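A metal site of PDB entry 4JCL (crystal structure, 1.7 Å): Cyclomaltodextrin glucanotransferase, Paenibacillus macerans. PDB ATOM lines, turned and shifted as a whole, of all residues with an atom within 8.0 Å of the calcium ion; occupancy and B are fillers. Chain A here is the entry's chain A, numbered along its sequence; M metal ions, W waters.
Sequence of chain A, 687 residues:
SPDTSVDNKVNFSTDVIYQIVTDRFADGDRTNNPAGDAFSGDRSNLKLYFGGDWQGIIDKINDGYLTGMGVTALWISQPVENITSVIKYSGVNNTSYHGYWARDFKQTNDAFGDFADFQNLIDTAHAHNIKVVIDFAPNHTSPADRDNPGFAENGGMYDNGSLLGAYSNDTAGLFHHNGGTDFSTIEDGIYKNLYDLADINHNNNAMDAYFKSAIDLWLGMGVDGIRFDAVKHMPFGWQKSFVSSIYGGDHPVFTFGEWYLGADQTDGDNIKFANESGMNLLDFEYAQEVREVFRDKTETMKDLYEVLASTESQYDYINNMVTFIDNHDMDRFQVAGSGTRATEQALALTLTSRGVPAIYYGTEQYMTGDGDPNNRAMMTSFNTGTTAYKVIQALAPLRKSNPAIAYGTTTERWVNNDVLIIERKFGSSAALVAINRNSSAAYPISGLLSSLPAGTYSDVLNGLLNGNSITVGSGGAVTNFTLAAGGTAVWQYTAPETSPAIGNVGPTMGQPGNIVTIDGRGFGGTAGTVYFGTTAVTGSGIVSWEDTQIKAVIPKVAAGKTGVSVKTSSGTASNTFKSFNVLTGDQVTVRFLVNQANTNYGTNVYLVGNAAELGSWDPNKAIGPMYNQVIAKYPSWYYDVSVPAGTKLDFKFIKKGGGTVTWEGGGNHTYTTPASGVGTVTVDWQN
Along chain A the residues within 4 Å of the calcium ion span positions 27 to 53.
The backbone NH (N) of Gly 51 sits at hydrogen-bond distance from the side-chain carboxylate (OD1) of Asp 23 (2.9 Å).
O of Ala 26 is in hydrogen-bond range of N of Asp 53, at 3.0 Å.
The backbone NH of Gln 55 sits close to the side-chain carboxylate of Asp 53 (3.4 Å).
OG1 of Thr 31 lies within hydrogen-bond range of OD1 of Asp 29, 2.5 Å away.
The side-chain carboxylate of Asp 53 is in hydrogen-bond range of the backbone NH of Gly 28 (2.9 Å).
The side-chain carboxylate (OD1) of Asp 53 is in hydrogen-bond range of the backbone NH (N) of Gly 56, 2.9 Å away.
O of Ala 111 lies close to ND2 of Asn 32 (3.5 Å).
The calcium ion is bound by OD1 of Asn 33 (2.3 Å), OD2 of Asp 53 (2.4 Å), OD1 of Asn 32 (2.5 Å), OD1 of Asp 27 (2.5 Å), O of Gly 51 (2.5 Å), O of Asp 29 (2.5 Å) and water W1 (2.6 Å).
The calcium ion has seven donor atoms within binding distance.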
ATOM      1  N   THR A  22      18.885  34.202  35.769  1.00  0.00           N
ATOM      2  CA  THR A  22      18.277  32.961  35.291  1.00  0.00           C
ATOM      3  C   THR A  22      18.302  32.804  33.772  1.00  0.00           C
ATOM      4  O   THR A  22      18.675  31.752  33.248  1.00  0.00           O
ATOM      5  CB  THR A  22      16.851  32.823  35.826  1.00  0.00           C
ATOM      6  OG1 THR A  22      16.881  32.917  37.249  1.00  0.00           O
ATOM      7  CG2 THR A  22      16.239  31.504  35.411  1.00  0.00           C
ATOM      8  N   ASP A  23      17.920  33.868  33.068  1.00  0.00           N
ATOM      9  CA  ASP A  23      17.817  33.787  31.608  1.00  0.00           C
ATOM     10  C   ASP A  23      19.171  33.567  30.939  1.00  0.00           C
ATOM     11  O   ASP A  23      19.234  33.163  29.779  1.00  0.00           O
ATOM     12  CB  ASP A  23      17.190  35.079  31.046  1.00  0.00           C
ATOM     13  CG  ASP A  23      16.997  35.009  29.538  1.00  0.00           C
ATOM     14  OD1 ASP A  23      16.199  34.160  29.115  1.00  0.00           O
ATOM     15  OD2 ASP A  23      17.637  35.793  28.801  1.00  0.00           O
ATOM     16  N   ALA A  26      21.529  28.745  31.986  1.00  0.00           N
ATOM     17  CA  ALA A  26      21.411  27.555  31.156  1.00  0.00           C
ATOM     18  C   ALA A  26      19.988  27.348  30.694  1.00  0.00           C
ATOM     19  O   ALA A  26      19.060  27.341  31.506  1.00  0.00           O
ATOM     20  CB  ALA A  26      21.898  26.329  31.915  1.00  0.00           C
ATOM     21  N   ASP A  27      19.813  27.179  29.390  1.00  0.00           N
ATOM     22  CA  ASP A  27      18.524  26.833  28.816  1.00  0.00           C
ATOM     23  C   ASP A  27      18.307  25.319  28.915  1.00  0.00           C
ATOM     24  O   ASP A  27      18.786  24.545  28.080  1.00  0.00           O
ATOM     25  CB  ASP A  27      18.456  27.328  27.368  1.00  0.00           C
ATOM     26  CG  ASP A  27      17.115  27.055  26.708  1.00  0.00           C
ATOM     27  OD1 ASP A  27      16.164  26.660  27.388  1.00  0.00           O
ATOM     28  OD2 ASP A  27      17.009  27.253  25.484  1.00  0.00           O
ATOM     29  N   GLY A  28      17.606  24.883  29.968  1.00  0.00           N
ATOM     30  CA  GLY A  28      17.398  23.463  30.208  1.00  0.00           C
ATOM     31  C   GLY A  28      16.133  22.940  29.534  1.00  0.00           C
ATOM     32  O   GLY A  28      15.944  21.730  29.388  1.00  0.00           O
ATOM     33  N   ASP A  29      15.270  23.845  29.114  1.00  0.00           N
ATOM     34  CA  ASP A  29      13.985  23.458  28.541  1.00  0.00           C
ATOM     35  C   ASP A  29      13.630  24.415  27.408  1.00  0.00           C
ATOM     36  O   ASP A  29      13.175  25.528  27.648  1.00  0.00           O
ATOM     37  CB  ASP A  29      12.902  23.462  29.625  1.00  0.00           C
ATOM     38  CG  ASP A  29      11.535  23.058  29.112  1.00  0.00           C
ATOM     39  OD1 ASP A  29      11.376  22.797  27.899  1.00  0.00           O
ATOM     40  OD2 ASP A  29      10.597  23.016  29.948  1.00  0.00           O
ATOM     41  N   ARG A  30      13.854  24.001  26.160  1.00  0.00           N
ATOM     42  CA  ARG A  30      13.628  24.933  25.054  1.00  0.00           C
ATOM     43  C   ARG A  30      12.138  25.223  24.847  1.00  0.00           C
ATOM     44  O   ARG A  30      11.781  26.203  24.179  1.00  0.00           O
ATOM     45  CB  ARG A  30      14.254  24.401  23.751  1.00  0.00           C
ATOM     46  CG  ARG A  30      15.775  24.395  23.768  1.00  0.00           C
ATOM     47  CD  ARG A  30      16.333  23.833  22.465  1.00  0.00           C
ATOM     48  NE  ARG A  30      17.793  23.795  22.474  1.00  0.00           N
ATOM     49  CZ  ARG A  30      18.534  23.369  21.462  1.00  0.00           C
ATOM     50  NH1 ARG A  30      17.960  22.918  20.353  1.00  0.00           N
ATOM     51  NH2 ARG A  30      19.864  23.372  21.560  1.00  0.00           N
ATOM     52  N   THR A  31      11.284  24.385  25.424  1.00  0.00           N
ATOM     53  CA  THR A  31       9.846  24.481  25.174  1.00  0.00           C
ATOM     54  C   THR A  31       9.190  25.648  25.926  1.00  0.00           C
ATOM     55  O   THR A  31       8.048  26.000  25.637  1.00  0.00           O
ATOM     56  CB  THR A  31       9.100  23.161  25.483  1.00  0.00           C
ATOM     57  OG1 THR A  31       9.092  22.903  26.889  1.00  0.00           O
ATOM     58  CG2 THR A  31       9.768  21.988  24.751  1.00  0.00           C
ATOM     59  N   ASN A  32       9.889  26.236  26.878  1.00  0.00           N
ATOM     60  CA  ASN A  32       9.352  27.426  27.507  1.00  0.00           C
ATOM     61  C   ASN A  32       9.986  28.742  26.995  1.00  0.00           C
ATOM     62  O   ASN A  32       9.702  29.806  27.525  1.00  0.00           O
ATOM     63  CB  ASN A  32       9.424  27.319  29.039  1.00  0.00           C
ATOM     64  CG  ASN A  32      10.830  27.187  29.543  1.00  0.00           C
ATOM     65  OD1 ASN A  32      11.760  27.638  28.885  1.00  0.00           O
ATOM     66  ND2 ASN A  32      11.012  26.544  30.699  1.00  0.00           N
ATOM     67  N   ASN A  33      10.823  28.650  25.968  1.00  0.00           N
ATOM     68  CA  ASN A  33      11.473  29.830  25.400  1.00  0.00           C
ATOM     69  C   ASN A  33      10.477  30.798  24.798  1.00  0.00           C
ATOM     70  O   ASN A  33       9.602  30.393  24.019  1.00  0.00           O
ATOM     71  CB  ASN A  33      12.485  29.449  24.321  1.00  0.00           C
ATOM     72  CG  ASN A  33      13.722  28.789  24.886  1.00  0.00           C
ATOM     73  OD1 ASN A  33      13.788  28.503  26.080  1.00  0.00           O
ATOM     74  ND2 ASN A  33      14.698  28.520  24.036  1.00  0.00           N
ATOM     75  N   PRO A  34      10.587  32.087  25.154  1.00  0.00           N
ATOM     76  CA  PRO A  34       9.813  33.097  24.429  1.00  0.00           C
ATOM     77  C   PRO A  34      10.196  33.042  22.959  1.00  0.00           C
ATOM     78  O   PRO A  34      11.176  32.384  22.611  1.00  0.00           O
ATOM     79  CB  PRO A  34      10.260  34.418  25.077  1.00  0.00           C
ATOM     80  CG  PRO A  34      10.663  34.003  26.479  1.00  0.00           C
ATOM     81  CD  PRO A  34      11.328  32.665  26.291  1.00  0.00           C
ATOM     82  N   PHE A  39      12.821  37.159  21.651  1.00  0.00           N
ATOM     83  CA  PHE A  39      13.848  36.137  21.827  1.00  0.00           C
ATOM     84  C   PHE A  39      15.014  36.370  20.886  1.00  0.00           C
ATOM     85  O   PHE A  39      14.828  36.714  19.723  1.00  0.00           O
ATOM     86  CB  PHE A  39      13.228  34.757  21.554  1.00  0.00           C
ATOM     87  CG  PHE A  39      14.156  33.589  21.808  1.00  0.00           C
ATOM     88  CD1 PHE A  39      14.372  33.139  23.099  1.00  0.00           C
ATOM     89  CD2 PHE A  39      14.774  32.929  20.758  1.00  0.00           C
ATOM     90  CE1 PHE A  39      15.209  32.053  23.349  1.00  0.00           C
ATOM     91  CE2 PHE A  39      15.608  31.840  20.995  1.00  0.00           C
ATOM     92  CZ  PHE A  39      15.832  31.401  22.289  1.00  0.00           C
ATOM     93  N   TYR A  49      15.062  37.791  25.713  1.00  0.00           N
ATOM     94  CA  TYR A  49      15.254  36.502  26.371  1.00  0.00           C
ATOM     95  C   TYR A  49      16.232  35.643  25.585  1.00  0.00           C
ATOM     96  O   TYR A  49      16.117  35.544  24.363  1.00  0.00           O
ATOM     97  CB  TYR A  49      13.933  35.750  26.498  1.00  0.00           C
ATOM     98  CG  TYR A  49      13.065  36.189  27.656  1.00  0.00           C
ATOM     99  CD1 TYR A  49      13.056  35.474  28.852  1.00  0.00           C
ATOM    100  CD2 TYR A  49      12.228  37.299  27.557  1.00  0.00           C
ATOM    101  CE1 TYR A  49      12.238  35.852  29.923  1.00  0.00           C
ATOM    102  CE2 TYR A  49      11.407  37.685  28.613  1.00  0.00           C
ATOM    103  CZ  TYR A  49      11.421  36.955  29.791  1.00  0.00           C
ATOM    104  OH  TYR A  49      10.626  37.334  30.864  1.00  0.00           O
ATOM    105  N   PHE A  50      17.183  35.025  26.284  1.00  0.00           N
ATOM    106  CA  PHE A  50      18.088  34.035  25.686  1.00  0.00           C
ATOM    107  C   PHE A  50      17.604  32.600  25.898  1.00  0.00           C
ATOM    108  O   PHE A  50      17.986  31.692  25.153  1.00  0.00           O
ATOM    109  CB  PHE A  50      19.518  34.149  26.233  1.00  0.00           C
ATOM    110  CG  PHE A  50      20.293  35.311  25.677  1.00  0.00           C
ATOM    111  CD1 PHE A  50      19.691  36.276  24.892  1.00  0.00           C
ATOM    112  CD2 PHE A  50      21.660  35.423  25.943  1.00  0.00           C
ATOM    113  CE1 PHE A  50      20.414  37.346  24.384  1.00  0.00           C
ATOM    114  CE2 PHE A  50      22.388  36.482  25.429  1.00  0.00           C
ATOM    115  CZ  PHE A  50      21.767  37.460  24.652  1.00  0.00           C
ATOM    116  N   GLY A  51      16.785  32.374  26.925  1.00  0.00           N
ATOM    117  CA  GLY A  51      16.212  31.057  27.163  1.00  0.00           C
ATOM    118  C   GLY A  51      16.588  30.351  28.457  1.00  0.00           C
ATOM    119  O   GLY A  51      16.064  29.274  28.756  1.00  0.00           O
ATOM    120  N   GLY A  52      17.491  30.934  29.250  1.00  0.00           N
ATOM    121  CA  GLY A  52      17.901  30.322  30.508  1.00  0.00           C
ATOM    122  C   GLY A  52      16.725  30.132  31.457  1.00  0.00           C
ATOM    123  O   GLY A  52      15.868  31.000  31.558  1.00  0.00           O
ATOM    124  N   ASP A  53      16.695  28.998  32.156  1.00  0.00           N
ATOM    125  CA  ASP A  53      15.511  28.676  32.972  1.00  0.00           C
ATOM    126  C   ASP A  53      15.826  27.847  34.220  1.00  0.00           C
ATOM    127  O   ASP A  53      16.977  27.535  34.505  1.00  0.00           O
ATOM    128  CB  ASP A  53      14.468  27.956  32.110  1.00  0.00           C
ATOM    129  CG  ASP A  53      15.047  26.762  31.374  1.00  0.00           C
ATOM    130  OD1 ASP A  53      15.895  26.042  31.934  1.00  0.00           O
ATOM    131  OD2 ASP A  53      14.663  26.545  30.213  1.00  0.00           O
ATOM    132  N   TRP A  54      14.775  27.487  34.960  1.00  0.00           N
ATOM    133  CA  TRP A  54      14.983  26.727  36.196  1.00  0.00           C
ATOM    134  C   TRP A  54      15.484  25.295  35.949  1.00  0.00           C
ATOM    135  O   TRP A  54      16.307  24.782  36.699  1.00  0.00           O
ATOM    136  CB  TRP A  54      13.730  26.737  37.074  1.00  0.00           C
ATOM    137  CG  TRP A  54      13.362  28.115  37.539  1.00  0.00           C
ATOM    138  CD1 TRP A  54      14.212  29.151  37.796  1.00  0.00           C
ATOM    139  CD2 TRP A  54      12.032  28.604  37.763  1.00  0.00           C
ATOM    140  NE1 TRP A  54      13.492  30.267  38.181  1.00  0.00           N
ATOM    141  CE2 TRP A  54      12.150  29.955  38.170  1.00  0.00           C
ATOM    142  CE3 TRP A  54      10.756  28.035  37.659  1.00  0.00           C
ATOM    143  CZ2 TRP A  54      11.046  30.739  38.482  1.00  0.00           C
ATOM    144  CZ3 TRP A  54       9.662  28.816  37.955  1.00  0.00           C
ATOM    145  CH2 TRP A  54       9.802  30.157  38.366  1.00  0.00           C
ATOM    146  N   GLN A  55      15.003  24.669  34.879  1.00  0.00           N
ATOM    147  CA  GLN A  55      15.477  23.335  34.520  1.00  0.00           C
ATOM    148  C   GLN A  55      16.991  23.352  34.273  1.00  0.00           C
ATOM    149  O   GLN A  55      17.698  22.385  34.595  1.00  0.00           O
ATOM    150  CB  GLN A  55      14.750  22.813  33.270  1.00  0.00           C
ATOM    151  CG  GLN A  55      15.159  21.395  32.901  1.00  0.00           C
ATOM    152  CD  GLN A  55      14.835  20.393  33.998  1.00  0.00           C
ATOM    153  OE1 GLN A  55      13.689  20.269  34.418  1.00  0.00           O
ATOM    154  NE2 GLN A  55      15.867  19.683  34.467  1.00  0.00           N
ATOM    155  N   GLY A  56      17.462  24.452  33.707  1.00  0.00           N
ATOM    156  CA  GLY A  56      18.886  24.619  33.441  1.00  0.00           C
ATOM    157  C   GLY A  56      19.688  24.687  34.722  1.00  0.00           C
ATOM    158  O   GLY A  56      20.779  24.125  34.809  1.00  0.00           O
ATOM    159  N   ASP A 110       6.650  32.291  33.080  1.00  0.00           N
ATOM    160  CA  ASP A 110       6.553  31.046  32.324  1.00  0.00           C
ATOM    161  C   ASP A 110       7.836  30.713  31.563  1.00  0.00           C
ATOM    162  O   ASP A 110       8.101  29.547  31.262  1.00  0.00           O
ATOM    163  CB  ASP A 110       5.360  31.086  31.373  1.00  0.00           C
ATOM    164  CG  ASP A 110       4.038  31.227  32.104  1.00  0.00           C
ATOM    165  OD1 ASP A 110       4.008  31.023  33.340  1.00  0.00           O
ATOM    166  OD2 ASP A 110       3.015  31.548  31.452  1.00  0.00           O
ATOM    167  N   ALA A 111       8.631  31.726  31.259  1.00  0.00           N
ATOM    168  CA  ALA A 111       9.897  31.481  30.565  1.00  0.00           C
ATOM    169  C   ALA A 111      10.852  30.709  31.446  1.00  0.00           C
ATOM    170  O   ALA A 111      11.704  29.965  30.939  1.00  0.00           O
ATOM    171  CB  ALA A 111      10.536  32.788  30.106  1.00  0.00           C
ATOM    172  N   PHE A 112      10.738  30.881  32.759  1.00  0.00           N
ATOM    173  CA  PHE A 112      11.628  30.203  33.687  1.00  0.00           C
ATOM    174  C   PHE A 112      11.094  28.812  34.050  1.00  0.00           C
ATOM    175  O   PHE A 112      11.863  27.885  34.281  1.00  0.00           O
ATOM    176  CB  PHE A 112      11.835  31.013  34.974  1.00  0.00           C
ATOM    177  CG  PHE A 112      12.476  32.368  34.772  1.00  0.00           C
ATOM    178  CD1 PHE A 112      13.237  32.631  33.638  1.00  0.00           C
ATOM    179  CD2 PHE A 112      12.321  33.362  35.726  1.00  0.00           C
ATOM    180  CE1 PHE A 112      13.819  33.889  33.457  1.00  0.00           C
ATOM    181  CE2 PHE A 112      12.903  34.619  35.544  1.00  0.00           C
ATOM    182  CZ  PHE A 112      13.664  34.873  34.413  1.00  0.00           C
ATOM    183  N   GLY A 113       9.781  28.675  34.090  1.00  0.00           N
ATOM    184  CA  GLY A 113       9.172  27.399  34.415  1.00  0.00           C
ATOM    185  C   GLY A 113       7.797  27.596  35.028  1.00  0.00           C
ATOM    186  O   GLY A 113       7.339  28.732  35.189  1.00  0.00           O
HETATM  187 CA    CA M   1      14.137  27.770  28.258  1.00  0.00          CA
HETATM  188  O   HOH W   1      13.166  30.089  28.836  1.00  0.00           O
